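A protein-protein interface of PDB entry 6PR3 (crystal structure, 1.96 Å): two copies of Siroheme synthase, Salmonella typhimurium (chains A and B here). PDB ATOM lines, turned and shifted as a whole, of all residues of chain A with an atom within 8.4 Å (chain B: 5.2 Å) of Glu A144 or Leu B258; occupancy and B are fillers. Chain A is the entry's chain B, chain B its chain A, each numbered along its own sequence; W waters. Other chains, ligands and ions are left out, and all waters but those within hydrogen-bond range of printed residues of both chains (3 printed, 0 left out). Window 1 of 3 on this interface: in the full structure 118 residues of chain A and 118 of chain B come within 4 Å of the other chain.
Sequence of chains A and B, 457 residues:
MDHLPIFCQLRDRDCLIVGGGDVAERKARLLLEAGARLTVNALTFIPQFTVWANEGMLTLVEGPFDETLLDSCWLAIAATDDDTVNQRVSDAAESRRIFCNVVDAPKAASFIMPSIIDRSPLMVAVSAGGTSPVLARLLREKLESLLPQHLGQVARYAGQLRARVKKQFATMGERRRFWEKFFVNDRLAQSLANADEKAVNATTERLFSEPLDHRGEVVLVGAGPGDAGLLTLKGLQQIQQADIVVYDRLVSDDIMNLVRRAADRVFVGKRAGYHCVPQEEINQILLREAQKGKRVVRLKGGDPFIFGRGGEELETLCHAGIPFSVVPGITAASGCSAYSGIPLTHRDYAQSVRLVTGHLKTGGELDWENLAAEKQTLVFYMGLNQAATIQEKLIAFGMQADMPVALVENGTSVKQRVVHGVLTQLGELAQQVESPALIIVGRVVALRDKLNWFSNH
O of Leu B231 sits at hydrogen-bond distance from N of Leu A233 (3.0 Å).
OE1 of Gln B240 is in hydrogen-bond range of NE of Arg A140 (2.8 Å).
N of Arg B260 lies within hydrogen-bond range of O of Ile B239 (3.1 Å).
NE2 of Gln B240 lies within hydrogen-bond range of O of Leu B258 (2.7 Å).
The side-chain hydroxyl (OG) of Ser A115 lies within hydrogen-bond range of the guanidinium group (NH1) of Arg A140 (3.2 Å).
The guanidinium group (NH2) of Arg A119 lies within salt-bridge range of the side-chain carboxylate (OE1) of Glu A144 (2.9 Å).
O of Lys A142 is in hydrogen-bond range of OG of Ser A145, 2.8 Å away.
The backbone carbonyl oxygen of Ser A145 is in hydrogen-bond range of the side-chain amide nitrogen of Gln A237 (3.0 Å).
CD of Arg A137 touches O of Gln B240 (3.8 Å).
Arg A140 touches Arg B260 (NH2 to CB, 3.4 Å).
Leu B236 touches Glu A141 (CD2 to O, 3.9 Å).
CB of Gln B240 touches OE2 of Glu A141, at 3.6 Å.
Glu A144 touches Leu B258 (OE1 to CD2, 3.6 Å).
CD2 of Leu B236 touches CB of Ser A145, 3.6 Å away.
Leu B258 touches Gln A149 (CD2 to NE2, 3.6 Å).
Leu A233 touches Ala B228 (CD1 to O, 3.6 Å).
Leu A233 touches Leu B236.
Printed residues of chain B within 4 Å of Arg A140: Gln B240 (2.8 Å) and Arg B260 (3.4 Å).
Of the printed residues of chain B, Glu A141 touches Leu B236 (3.9 Å) and Gln B240 (3.6 Å).
Printed residues of chain B within 4 Å of Gln A149: Leu B258 (3.6 Å).
Gln A237 touches none of the printed residues of chain B.
Of the printed residues of chain A, Leu B236 touches Glu A141 (3.9 Å), Ser A145 (3.6 Å) and Leu A233 (3.8 Å).
Leu B258 touches just these residues of chain A: Glu A144 (3.6 Å) and Gln A149 (3.6 Å).
The nearest residue of chain A that does not touch Leu B258 is Leu A233 (4.02 Å).
Of the 23 printed residues of chain A, 7 touch a printed residue of chain B.
Hydrophobic or aromatic side chains of chain A that line the printed part of chain B: Leu A233.
Hydrophobic or aromatic side chains of chain B within 4 Å of the printed part of chain A: Leu B236 and Leu B258.
Among the printed residues, 11 pairs touch across the chains.
Among the printed residues, no Asp or Glu carboxylate lies within 4 Å of a Lys or Arg side-chain nitrogen of the other chain.
1 position is printed for both chains.
Of the 11 pairs that touch across the chains among the printed residues, none has its exchanged pair printed and touching as well.
Water W2 lies within hydrogen-bond range of the side-chain amide nitrogen (NE2) of Gln A149 (2.5 Å) and the backbone carbonyl oxygen (O) of Asp B254 (2.6 Å).
Water W1 bridges NE2 of Gln B240 (3.0 Å) and NE of Arg A140 (3.3 Å).
Water W3 lies within hydrogen-bond range of the guanidinium group (NH1) of Arg B260 (3.2 Å) and the guanidinium group (NH1) of Arg A140 (3.3 Å).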
ATOM      1  N   SER A 115      11.589  -6.026 -22.482  1.00  0.00           N
ATOM      2  CA  SER A 115      12.192  -4.747 -22.126  1.00  0.00           C
ATOM      3  C   SER A 115      12.690  -4.082 -23.399  1.00  0.00           C
ATOM      4  O   SER A 115      13.210  -4.748 -24.299  1.00  0.00           O
ATOM      5  CB  SER A 115      13.362  -4.935 -21.159  1.00  0.00           C
ATOM      6  OG  SER A 115      12.926  -5.178 -19.842  1.00  0.00           O
ATOM      7  N   ILE A 116      12.524  -2.769 -23.494  1.00  0.00           N
ATOM      8  CA  ILE A 116      12.846  -2.054 -24.726  1.00  0.00           C
ATOM      9  C   ILE A 116      13.835  -0.937 -24.441  1.00  0.00           C
ATOM     10  O   ILE A 116      13.651  -0.163 -23.495  1.00  0.00           O
ATOM     11  CB  ILE A 116      11.578  -1.495 -25.394  1.00  0.00           C
ATOM     12  CG1 ILE A 116      10.684  -2.640 -25.873  1.00  0.00           C
ATOM     13  CG2 ILE A 116      11.932  -0.640 -26.616  1.00  0.00           C
ATOM     14  CD1 ILE A 116       9.248  -2.194 -26.173  1.00  0.00           C
ATOM     15  N   ILE A 117      14.878  -0.852 -25.265  1.00  0.00           N
ATOM     16  CA  ILE A 117      15.772   0.302 -25.274  1.00  0.00           C
ATOM     17  C   ILE A 117      15.559   0.998 -26.605  1.00  0.00           C
ATOM     18  O   ILE A 117      15.883   0.444 -27.662  1.00  0.00           O
ATOM     19  CB  ILE A 117      17.240  -0.080 -25.079  1.00  0.00           C
ATOM     20  CG1 ILE A 117      17.452  -0.721 -23.703  1.00  0.00           C
ATOM     21  CG2 ILE A 117      18.100   1.183 -25.179  1.00  0.00           C
ATOM     22  CD1 ILE A 117      17.390  -2.240 -23.707  1.00  0.00           C
ATOM     23  N   ASP A 118      14.991   2.192 -26.553  1.00  0.00           N
ATOM     24  CA  ASP A 118      14.544   2.917 -27.734  1.00  0.00           C
ATOM     25  C   ASP A 118      15.600   3.963 -28.084  1.00  0.00           C
ATOM     26  O   ASP A 118      15.837   4.900 -27.318  1.00  0.00           O
ATOM     27  CB  ASP A 118      13.181   3.557 -27.467  1.00  0.00           C
ATOM     28  CG  ASP A 118      12.662   4.370 -28.645  1.00  0.00           C
ATOM     29  OD1 ASP A 118      13.273   4.342 -29.729  1.00  0.00           O
ATOM     30  OD2 ASP A 118      11.626   5.040 -28.473  1.00  0.00           O
ATOM     31  N   ARG A 119      16.230   3.790 -29.233  1.00  0.00           N
ATOM     32  CA  ARG A 119      17.096   4.786 -29.855  1.00  0.00           C
ATOM     33  C   ARG A 119      16.716   4.942 -31.319  1.00  0.00           C
ATOM     34  O   ARG A 119      17.585   4.964 -32.203  1.00  0.00           O
ATOM     35  CB  ARG A 119      18.567   4.397 -29.736  1.00  0.00           C
ATOM     36  CG  ARG A 119      19.062   4.242 -28.309  1.00  0.00           C
ATOM     37  CD  ARG A 119      19.110   5.598 -27.585  1.00  0.00           C
ATOM     38  NE  ARG A 119      19.754   5.443 -26.291  1.00  0.00           N
ATOM     39  CZ  ARG A 119      19.145   5.016 -25.191  1.00  0.00           C
ATOM     40  NH1 ARG A 119      17.850   4.745 -25.209  1.00  0.00           N
ATOM     41  NH2 ARG A 119      19.840   4.884 -24.061  1.00  0.00           N
ATOM     42  N   VAL A 124      16.624  -2.010 -29.266  1.00  0.00           N
ATOM     43  CA  VAL A 124      17.112  -3.222 -28.615  1.00  0.00           C
ATOM     44  C   VAL A 124      15.989  -3.735 -27.731  1.00  0.00           C
ATOM     45  O   VAL A 124      15.308  -2.949 -27.060  1.00  0.00           O
ATOM     46  CB  VAL A 124      18.387  -2.972 -27.775  1.00  0.00           C
ATOM     47  CG1 VAL A 124      18.865  -4.274 -27.094  1.00  0.00           C
ATOM     48  CG2 VAL A 124      19.496  -2.373 -28.663  1.00  0.00           C
ATOM     49  N   ARG A 137      15.178  -6.511 -16.717  1.00  0.00           N
ATOM     50  CA  ARG A 137      15.362  -5.146 -16.224  1.00  0.00           C
ATOM     51  C   ARG A 137      16.832  -4.828 -15.958  1.00  0.00           C
ATOM     52  O   ARG A 137      17.301  -3.724 -16.272  1.00  0.00           O
ATOM     53  CB  ARG A 137      14.547  -4.942 -14.943  1.00  0.00           C
ATOM     54  CG  ARG A 137      14.716  -3.578 -14.313  1.00  0.00           C
ATOM     55  CD  ARG A 137      14.531  -3.628 -12.813  1.00  0.00           C
ATOM     56  NE  ARG A 137      15.802  -3.780 -12.132  1.00  0.00           N
ATOM     57  CZ  ARG A 137      15.945  -4.190 -10.879  1.00  0.00           C
ATOM     58  NH1 ARG A 137      14.882  -4.507 -10.145  1.00  0.00           N
ATOM     59  NH2 ARG A 137      17.163  -4.283 -10.360  1.00  0.00           N
ATOM     60  N   LEU A 138      17.554  -5.744 -15.298  1.00  0.00           N
ATOM     61  CA  LEU A 138      18.977  -5.521 -15.031  1.00  0.00           C
ATOM     62  C   LEU A 138      19.758  -5.343 -16.319  1.00  0.00           C
ATOM     63  O   LEU A 138      20.660  -4.497 -16.399  1.00  0.00           O
ATOM     64  CB  LEU A 138      19.554  -6.679 -14.217  1.00  0.00           C
ATOM     65  CG  LEU A 138      19.092  -6.765 -12.760  1.00  0.00           C
ATOM     66  CD1 LEU A 138      19.347  -8.157 -12.209  1.00  0.00           C
ATOM     67  CD2 LEU A 138      19.813  -5.716 -11.911  1.00  0.00           C
ATOM     68  N   LEU A 139      19.402  -6.091 -17.360  1.00  0.00           N
ATOM     69  CA  LEU A 139      20.091  -5.915 -18.635  1.00  0.00           C
ATOM     70  C   LEU A 139      19.685  -4.604 -19.297  1.00  0.00           C
ATOM     71  O   LEU A 139      20.539  -3.883 -19.834  1.00  0.00           O
ATOM     72  CB  LEU A 139      19.797  -7.107 -19.557  1.00  0.00           C
ATOM     73  CG  LEU A 139      20.439  -8.405 -19.058  1.00  0.00           C
ATOM     74  CD1 LEU A 139      19.929  -9.620 -19.814  1.00  0.00           C
ATOM     75  CD2 LEU A 139      21.963  -8.319 -19.140  1.00  0.00           C
ATOM     76  N   ARG A 140      18.383  -4.287 -19.281  1.00  0.00           N
ATOM     77  CA  ARG A 140      17.909  -3.038 -19.867  1.00  0.00           C
ATOM     78  C   ARG A 140      18.637  -1.850 -19.245  1.00  0.00           C
ATOM     79  O   ARG A 140      19.118  -0.953 -19.952  1.00  0.00           O
ATOM     80  CB  ARG A 140      16.389  -2.912 -19.674  1.00  0.00           C
ATOM     81  CG  ARG A 140      15.762  -1.691 -20.387  1.00  0.00           C
ATOM     82  CD  ARG A 140      14.314  -1.427 -19.969  1.00  0.00           C
ATOM     83  NE  ARG A 140      14.222  -0.966 -18.580  1.00  0.00           N
ATOM     84  CZ  ARG A 140      13.528  -1.583 -17.622  1.00  0.00           C
ATOM     85  NH1 ARG A 140      12.850  -2.689 -17.898  1.00  0.00           N
ATOM     86  NH2 ARG A 140      13.507  -1.095 -16.387  1.00  0.00           N
ATOM     87  N   GLU A 141      18.701  -1.827 -17.911  1.00  0.00           N
ATOM     88  CA  GLU A 141      19.497  -0.877 -17.136  1.00  0.00           C
ATOM     89  C   GLU A 141      20.899  -0.679 -17.703  1.00  0.00           C
ATOM     90  O   GLU A 141      21.331   0.452 -17.983  1.00  0.00           O
ATOM     91  CB  GLU A 141      19.581  -1.398 -15.693  1.00  0.00           C
ATOM     92  CG  GLU A 141      19.491  -0.381 -14.601  1.00  0.00           C
ATOM     93  CD  GLU A 141      19.397  -1.036 -13.235  1.00  0.00           C
ATOM     94  OE1 GLU A 141      20.233  -1.918 -12.925  1.00  0.00           O
ATOM     95  OE2 GLU A 141      18.483  -0.675 -12.472  1.00  0.00           O
ATOM     96  N   LYS A 142      21.631  -1.787 -17.839  1.00  0.00           N
ATOM     97  CA  LYS A 142      22.992  -1.755 -18.378  1.00  0.00           C
ATOM     98  C   LYS A 142      23.026  -1.147 -19.773  1.00  0.00           C
ATOM     99  O   LYS A 142      23.892  -0.314 -20.087  1.00  0.00           O
ATOM    100  CB  LYS A 142      23.570  -3.171 -18.414  1.00  0.00           C
ATOM    101  CG  LYS A 142      25.066  -3.287 -18.215  1.00  0.00           C
ATOM    102  CD  LYS A 142      25.551  -4.660 -18.691  1.00  0.00           C
ATOM    103  CE  LYS A 142      26.777  -5.162 -17.931  1.00  0.00           C
ATOM    104  NZ  LYS A 142      26.737  -6.647 -17.735  1.00  0.00           N
ATOM    105  N   LEU A 143      22.113  -1.590 -20.639  1.00  0.00           N
ATOM    106  CA  LEU A 143      22.099  -1.124 -22.017  1.00  0.00           C
ATOM    107  C   LEU A 143      21.745   0.354 -22.089  1.00  0.00           C
ATOM    108  O   LEU A 143      22.286   1.086 -22.928  1.00  0.00           O
ATOM    109  CB  LEU A 143      21.111  -1.965 -22.834  1.00  0.00           C
ATOM    110  CG  LEU A 143      21.447  -3.452 -22.910  1.00  0.00           C
ATOM    111  CD1 LEU A 143      20.437  -4.243 -23.765  1.00  0.00           C
ATOM    112  CD2 LEU A 143      22.852  -3.609 -23.446  1.00  0.00           C
ATOM    113  N   GLU A 144      20.843   0.810 -21.211  1.00  0.00           N
ATOM    114  CA  GLU A 144      20.495   2.224 -21.191  1.00  0.00           C
ATOM    115  C   GLU A 144      21.726   3.080 -20.919  1.00  0.00           C
ATOM    116  O   GLU A 144      21.914   4.121 -21.555  1.00  0.00           O
ATOM    117  CB  GLU A 144      19.400   2.504 -20.153  1.00  0.00           C
ATOM    118  CG  GLU A 144      18.003   1.982 -20.546  1.00  0.00           C
ATOM    119  CD  GLU A 144      17.351   2.768 -21.685  1.00  0.00           C
ATOM    120  OE1 GLU A 144      17.978   3.707 -22.224  1.00  0.00           O
ATOM    121  OE2 GLU A 144      16.200   2.431 -22.047  1.00  0.00           O
ATOM    122  N   SER A 145      22.576   2.656 -19.975  1.00  0.00           N
ATOM    123  CA  SER A 145      23.766   3.427 -19.643  1.00  0.00           C
ATOM    124  C   SER A 145      24.805   3.413 -20.761  1.00  0.00           C
ATOM    125  O   SER A 145      25.640   4.327 -20.827  1.00  0.00           O
ATOM    126  CB  SER A 145      24.394   2.899 -18.358  1.00  0.00           C
ATOM    127  OG  SER A 145      25.124   1.704 -18.604  1.00  0.00           O
ATOM    128  N   LEU A 146      24.775   2.402 -21.627  1.00  0.00           N
ATOM    129  CA  LEU A 146      25.805   2.200 -22.641  1.00  0.00           C
ATOM    130  C   LEU A 146      25.477   2.866 -23.968  1.00  0.00           C
ATOM    131  O   LEU A 146      26.396   3.266 -24.697  1.00  0.00           O
ATOM    132  CB  LEU A 146      26.020   0.699 -22.878  1.00  0.00           C
ATOM    133  CG  LEU A 146      26.707  -0.042 -21.730  1.00  0.00           C
ATOM    134  CD1 LEU A 146      27.021  -1.483 -22.126  1.00  0.00           C
ATOM    135  CD2 LEU A 146      27.965   0.684 -21.277  1.00  0.00           C
ATOM    136  N   LEU A 147      24.190   2.989 -24.304  1.00  0.00           N
ATOM    137  CA  LEU A 147      23.802   3.497 -25.609  1.00  0.00           C
ATOM    138  C   LEU A 147      23.564   4.997 -25.508  1.00  0.00           C
ATOM    139  O   LEU A 147      22.620   5.418 -24.819  1.00  0.00           O
ATOM    140  CB  LEU A 147      22.561   2.783 -26.107  1.00  0.00           C
ATOM    141  CG  LEU A 147      22.825   1.316 -26.442  1.00  0.00           C
ATOM    142  CD1 LEU A 147      21.545   0.635 -26.878  1.00  0.00           C
ATOM    143  CD2 LEU A 147      23.890   1.218 -27.537  1.00  0.00           C
ATOM    144  N   PRO A 148      24.371   5.824 -26.168  1.00  0.00           N
ATOM    145  CA  PRO A 148      24.169   7.277 -26.106  1.00  0.00           C
ATOM    146  C   PRO A 148      22.756   7.684 -26.514  1.00  0.00           C
ATOM    147  O   PRO A 148      22.130   7.064 -27.380  1.00  0.00           O
ATOM    148  CB  PRO A 148      25.222   7.818 -27.077  1.00  0.00           C
ATOM    149  CG  PRO A 148      26.275   6.734 -27.146  1.00  0.00           C
ATOM    150  CD  PRO A 148      25.533   5.439 -26.993  1.00  0.00           C
ATOM    151  N   GLN A 149      22.238   8.723 -25.851  1.00  0.00           N
ATOM    152  CA  GLN A 149      20.829   9.083 -26.031  1.00  0.00           C
ATOM    153  C   GLN A 149      20.513   9.487 -27.469  1.00  0.00           C
ATOM    154  O   GLN A 149      19.369   9.345 -27.905  1.00  0.00           O
ATOM    155  CB  GLN A 149      20.433  10.217 -25.081  1.00  0.00           C
ATOM    156  CG  GLN A 149      18.998  10.108 -24.531  1.00  0.00           C
ATOM    157  CD  GLN A 149      18.828   8.972 -23.522  1.00  0.00           C
ATOM    158  OE1 GLN A 149      19.750   8.645 -22.768  1.00  0.00           O
ATOM    159  NE2 GLN A 149      17.643   8.360 -23.513  1.00  0.00           N
ATOM    160  N   LEU A 233      26.523   9.024 -17.248  1.00  0.00           N
ATOM    161  CA  LEU A 233      26.360   8.116 -18.386  1.00  0.00           C
ATOM    162  C   LEU A 233      27.307   8.503 -19.509  1.00  0.00           C
ATOM    163  O   LEU A 233      27.997   7.657 -20.081  1.00  0.00           O
ATOM    164  CB  LEU A 233      24.920   8.139 -18.904  1.00  0.00           C
ATOM    165  CG  LEU A 233      23.805   8.067 -17.845  1.00  0.00           C
ATOM    166  CD1 LEU A 233      22.450   7.959 -18.511  1.00  0.00           C
ATOM    167  CD2 LEU A 233      24.031   6.912 -16.911  1.00  0.00           C
ATOM    168  N   LYS A 234      27.349   9.793 -19.838  1.00  0.00           N
ATOM    169  CA  LYS A 234      28.229  10.237 -20.909  1.00  0.00           C
ATOM    170  C   LYS A 234      29.698  10.005 -20.568  1.00  0.00           C
ATOM    171  O   LYS A 234      30.483   9.608 -21.435  1.00  0.00           O
ATOM    172  CB  LYS A 234      27.979  11.708 -21.242  1.00  0.00           C
ATOM    173  CG  LYS A 234      28.667  12.093 -22.575  1.00  0.00           C
ATOM    174  CD  LYS A 234      28.391  13.515 -23.021  1.00  0.00           C
ATOM    175  CE  LYS A 234      28.845  13.724 -24.461  1.00  0.00           C
ATOM    176  NZ  LYS A 234      28.760  15.159 -24.869  1.00  0.00           N
ATOM    177  N   LEU A 236      30.913   7.583 -18.670  1.00  0.00           N
ATOM    178  CA  LEU A 236      31.128   6.152 -18.895  1.00  0.00           C
ATOM    179  C   LEU A 236      31.226   5.826 -20.388  1.00  0.00           C
ATOM    180  O   LEU A 236      32.060   5.013 -20.807  1.00  0.00           O
ATOM    181  CB  LEU A 236      29.991   5.352 -18.252  1.00  0.00           C
ATOM    182  CG  LEU A 236      30.014   3.856 -18.566  1.00  0.00           C
ATOM    183  CD1 LEU A 236      31.215   3.221 -17.886  1.00  0.00           C
ATOM    184  CD2 LEU A 236      28.713   3.167 -18.125  1.00  0.00           C
ATOM    185  N   GLN A 237      30.346   6.411 -21.199  1.00  0.00           N
ATOM    186  CA  GLN A 237      30.377   6.147 -22.635  1.00  0.00           C
ATOM    187  C   GLN A 237      31.700   6.586 -23.252  1.00  0.00           C
ATOM    188  O   GLN A 237      32.261   5.885 -24.107  1.00  0.00           O
ATOM    189  CB  GLN A 237      29.198   6.849 -23.302  1.00  0.00           C
ATOM    190  CG  GLN A 237      27.845   6.222 -22.915  1.00  0.00           C
ATOM    191  CD  GLN A 237      26.677   7.186 -23.096  1.00  0.00           C
ATOM    192  OE1 GLN A 237      26.806   8.233 -23.722  1.00  0.00           O
ATOM    193  NE2 GLN A 237      25.535   6.836 -22.538  1.00  0.00           N
ATOM    194  N   ALA B 228      20.415  14.310 -20.744  1.00  0.00           N
ATOM    195  CA  ALA B 228      20.197  13.023 -20.095  1.00  0.00           C
ATOM    196  C   ALA B 228      21.498  12.270 -19.882  1.00  0.00           C
ATOM    197  O   ALA B 228      21.580  11.434 -18.974  1.00  0.00           O
ATOM    198  CB  ALA B 228      19.226  12.164 -20.901  1.00  0.00           C
ATOM    199  N   LEU B 231      23.018  12.398 -16.179  1.00  0.00           N
ATOM    200  CA  LEU B 231      22.587  11.608 -15.031  1.00  0.00           C
ATOM    201  C   LEU B 231      23.744  10.722 -14.568  1.00  0.00           C
ATOM    202  O   LEU B 231      24.567  10.282 -15.376  1.00  0.00           O
ATOM    203  CB  LEU B 231      21.384  10.742 -15.416  1.00  0.00           C
ATOM    204  CG  LEU B 231      20.618   9.993 -14.314  1.00  0.00           C
ATOM    205  CD1 LEU B 231      20.023  10.941 -13.267  1.00  0.00           C
ATOM    206  CD2 LEU B 231      19.515   9.109 -14.941  1.00  0.00           C
ATOM    207  N   LEU B 236      20.692   6.634 -12.563  1.00  0.00           N
ATOM    208  CA  LEU B 236      19.978   5.830 -13.555  1.00  0.00           C
ATOM    209  C   LEU B 236      19.478   4.526 -12.942  1.00  0.00           C
ATOM    210  O   LEU B 236      18.326   4.114 -13.181  1.00  0.00           O
ATOM    211  CB  LEU B 236      20.888   5.547 -14.770  1.00  0.00           C
ATOM    212  CG  LEU B 236      20.293   4.565 -15.803  1.00  0.00           C
ATOM    213  CD1 LEU B 236      19.037   5.131 -16.443  1.00  0.00           C
ATOM    214  CD2 LEU B 236      21.321   4.190 -16.887  1.00  0.00           C
ATOM    215  N   ILE B 239      16.246   5.240 -11.013  1.00  0.00           N
ATOM    216  CA  ILE B 239      14.998   5.486 -11.743  1.00  0.00           C
ATOM    217  C   ILE B 239      14.608   4.326 -12.648  1.00  0.00           C
ATOM    218  O   ILE B 239      13.433   4.224 -13.049  1.00  0.00           O
ATOM    219  CB  ILE B 239      15.033   6.776 -12.575  1.00  0.00           C
ATOM    220  CG1 ILE B 239      16.105   6.716 -13.661  1.00  0.00           C
ATOM    221  CG2 ILE B 239      15.200   8.009 -11.672  1.00  0.00           C
ATOM    222  CD1 ILE B 239      16.205   7.995 -14.450  1.00  0.00           C
ATOM    223  N   GLN B 240      15.558   3.449 -12.990  1.00  0.00           N
ATOM    224  CA  GLN B 240      15.250   2.210 -13.697  1.00  0.00           C
ATOM    225  C   GLN B 240      14.625   1.151 -12.792  1.00  0.00           C
ATOM    226  O   GLN B 240      14.145   0.127 -13.301  1.00  0.00           O
ATOM    227  CB  GLN B 240      16.524   1.673 -14.359  1.00  0.00           C
ATOM    228  CG  GLN B 240      16.849   2.374 -15.686  1.00  0.00           C
ATOM    229  CD  GLN B 240      15.925   1.924 -16.811  1.00  0.00           C
ATOM    230  OE1 GLN B 240      15.778   0.726 -17.056  1.00  0.00           O
ATOM    231  NE2 GLN B 240      15.289   2.884 -17.491  1.00  0.00           N
ATOM    232  N   ASP B 254      13.981  14.445 -21.432  1.00  0.00           N
ATOM    233  CA  ASP B 254      14.917  13.383 -21.783  1.00  0.00           C
ATOM    234  C   ASP B 254      15.304  12.549 -20.569  1.00  0.00           C
ATOM    235  O   ASP B 254      15.466  11.328 -20.677  1.00  0.00           O
ATOM    236  CB  ASP B 254      16.152  13.979 -22.453  1.00  0.00           C
ATOM    237  CG  ASP B 254      15.949  14.189 -23.943  1.00  0.00           C
ATOM    238  OD1 ASP B 254      15.094  13.483 -24.523  1.00  0.00           O
ATOM    239  OD2 ASP B 254      16.639  15.042 -24.536  1.00  0.00           O
ATOM    240  N   ILE B 255      15.457  13.178 -19.404  1.00  0.00           N
ATOM    241  CA  ILE B 255      15.690  12.394 -18.196  1.00  0.00           C
ATOM    242  C   ILE B 255      14.465  11.530 -17.902  1.00  0.00           C
ATOM    243  O   ILE B 255      14.577  10.318 -17.661  1.00  0.00           O
ATOM    244  CB  ILE B 255      16.042  13.313 -17.010  1.00  0.00           C
ATOM    245  CG1 ILE B 255      17.423  13.970 -17.189  1.00  0.00           C
ATOM    246  CG2 ILE B 255      15.962  12.531 -15.719  1.00  0.00           C
ATOM    247  CD1 ILE B 255      18.587  13.115 -16.727  1.00  0.00           C
ATOM    248  N   MET B 256      13.263  12.130 -17.968  1.00  0.00           N
ATOM    249  CA  MET B 256      12.050  11.356 -17.704  1.00  0.00           C
ATOM    250  C   MET B 256      11.923  10.171 -18.653  1.00  0.00           C
ATOM    251  O   MET B 256      11.321   9.151 -18.298  1.00  0.00           O
ATOM    252  CB  MET B 256      10.806  12.241 -17.803  1.00  0.00           C
ATOM    253  CG  MET B 256      10.651  13.210 -16.637  1.00  0.00           C
ATOM    254  SD  MET B 256      10.865  12.437 -15.011  1.00  0.00           S
ATOM    255  CE  MET B 256       9.382  11.420 -14.922  1.00  0.00           C
ATOM    256  N   ASN B 257      12.493  10.273 -19.855  1.00  0.00           N
ATOM    257  CA  ASN B 257      12.495   9.122 -20.749  1.00  0.00           C
ATOM    258  C   ASN B 257      13.288   7.938 -20.197  1.00  0.00           C
ATOM    259  O   ASN B 257      13.093   6.818 -20.678  1.00  0.00           O
ATOM    260  CB  ASN B 257      13.035   9.513 -22.131  1.00  0.00           C
ATOM    261  CG  ASN B 257      12.007  10.245 -22.973  1.00  0.00           C
ATOM    262  OD1 ASN B 257      10.817  10.244 -22.660  1.00  0.00           O
ATOM    263  ND2 ASN B 257      12.463  10.869 -24.051  1.00  0.00           N
ATOM    264  N   LEU B 258      14.163   8.146 -19.199  1.00  0.00           N
ATOM    265  CA  LEU B 258      14.931   7.057 -18.596  1.00  0.00           C
ATOM    266  C   LEU B 258      14.256   6.439 -17.377  1.00  0.00           C
ATOM    267  O   LEU B 258      14.784   5.477 -16.805  1.00  0.00           O
ATOM    268  CB  LEU B 258      16.330   7.552 -18.198  1.00  0.00           C
ATOM    269  CG  LEU B 258      17.207   7.938 -19.389  1.00  0.00           C
ATOM    270  CD1 LEU B 258      18.493   8.563 -18.911  1.00  0.00           C
ATOM    271  CD2 LEU B 258      17.475   6.724 -20.264  1.00  0.00           C
ATOM    272  N   VAL B 259      13.138   6.991 -16.929  1.00  0.00           N
ATOM    273  CA  VAL B 259      12.376   6.361 -15.863  1.00  0.00           C
ATOM    274  C   VAL B 259      11.704   5.122 -16.434  1.00  0.00           C
ATOM    275  O   VAL B 259      11.075   5.178 -17.500  1.00  0.00           O
ATOM    276  CB  VAL B 259      11.352   7.352 -15.290  1.00  0.00           C
ATOM    277  CG1 VAL B 259      10.463   6.683 -14.255  1.00  0.00           C
ATOM    278  CG2 VAL B 259      12.064   8.600 -14.713  1.00  0.00           C
ATOM    279  N   ARG B 260      11.856   3.987 -15.755  1.00  0.00           N
ATOM    280  CA  ARG B 260      11.323   2.749 -16.309  1.00  0.00           C
ATOM    281  C   ARG B 260       9.820   2.873 -16.544  1.00  0.00           C
ATOM    282  O   ARG B 260       9.110   3.576 -15.821  1.00  0.00           O
ATOM    283  CB  ARG B 260      11.642   1.568 -15.397  1.00  0.00           C
ATOM    284  CG  ARG B 260      10.976   1.594 -14.063  1.00  0.00           C
ATOM    285  CD  ARG B 260      10.991   0.199 -13.476  1.00  0.00           C
ATOM    286  NE  ARG B 260      10.301   0.145 -12.203  1.00  0.00           N
ATOM    287  CZ  ARG B 260       9.827  -0.970 -11.660  1.00  0.00           C
ATOM    288  NH1 ARG B 260       9.985  -2.129 -12.286  1.00  0.00           N
ATOM    289  NH2 ARG B 260       9.201  -0.925 -10.491  1.00  0.00           N
HETATM  290  O   HOH W   1      13.487   1.991 -19.733  1.00  0.00           O
HETATM  291  O   HOH W   2      16.258  10.310 -22.892  1.00  0.00           O
HETATM  292  O   HOH W   3      10.940  -3.011 -15.192  1.00  0.00           O
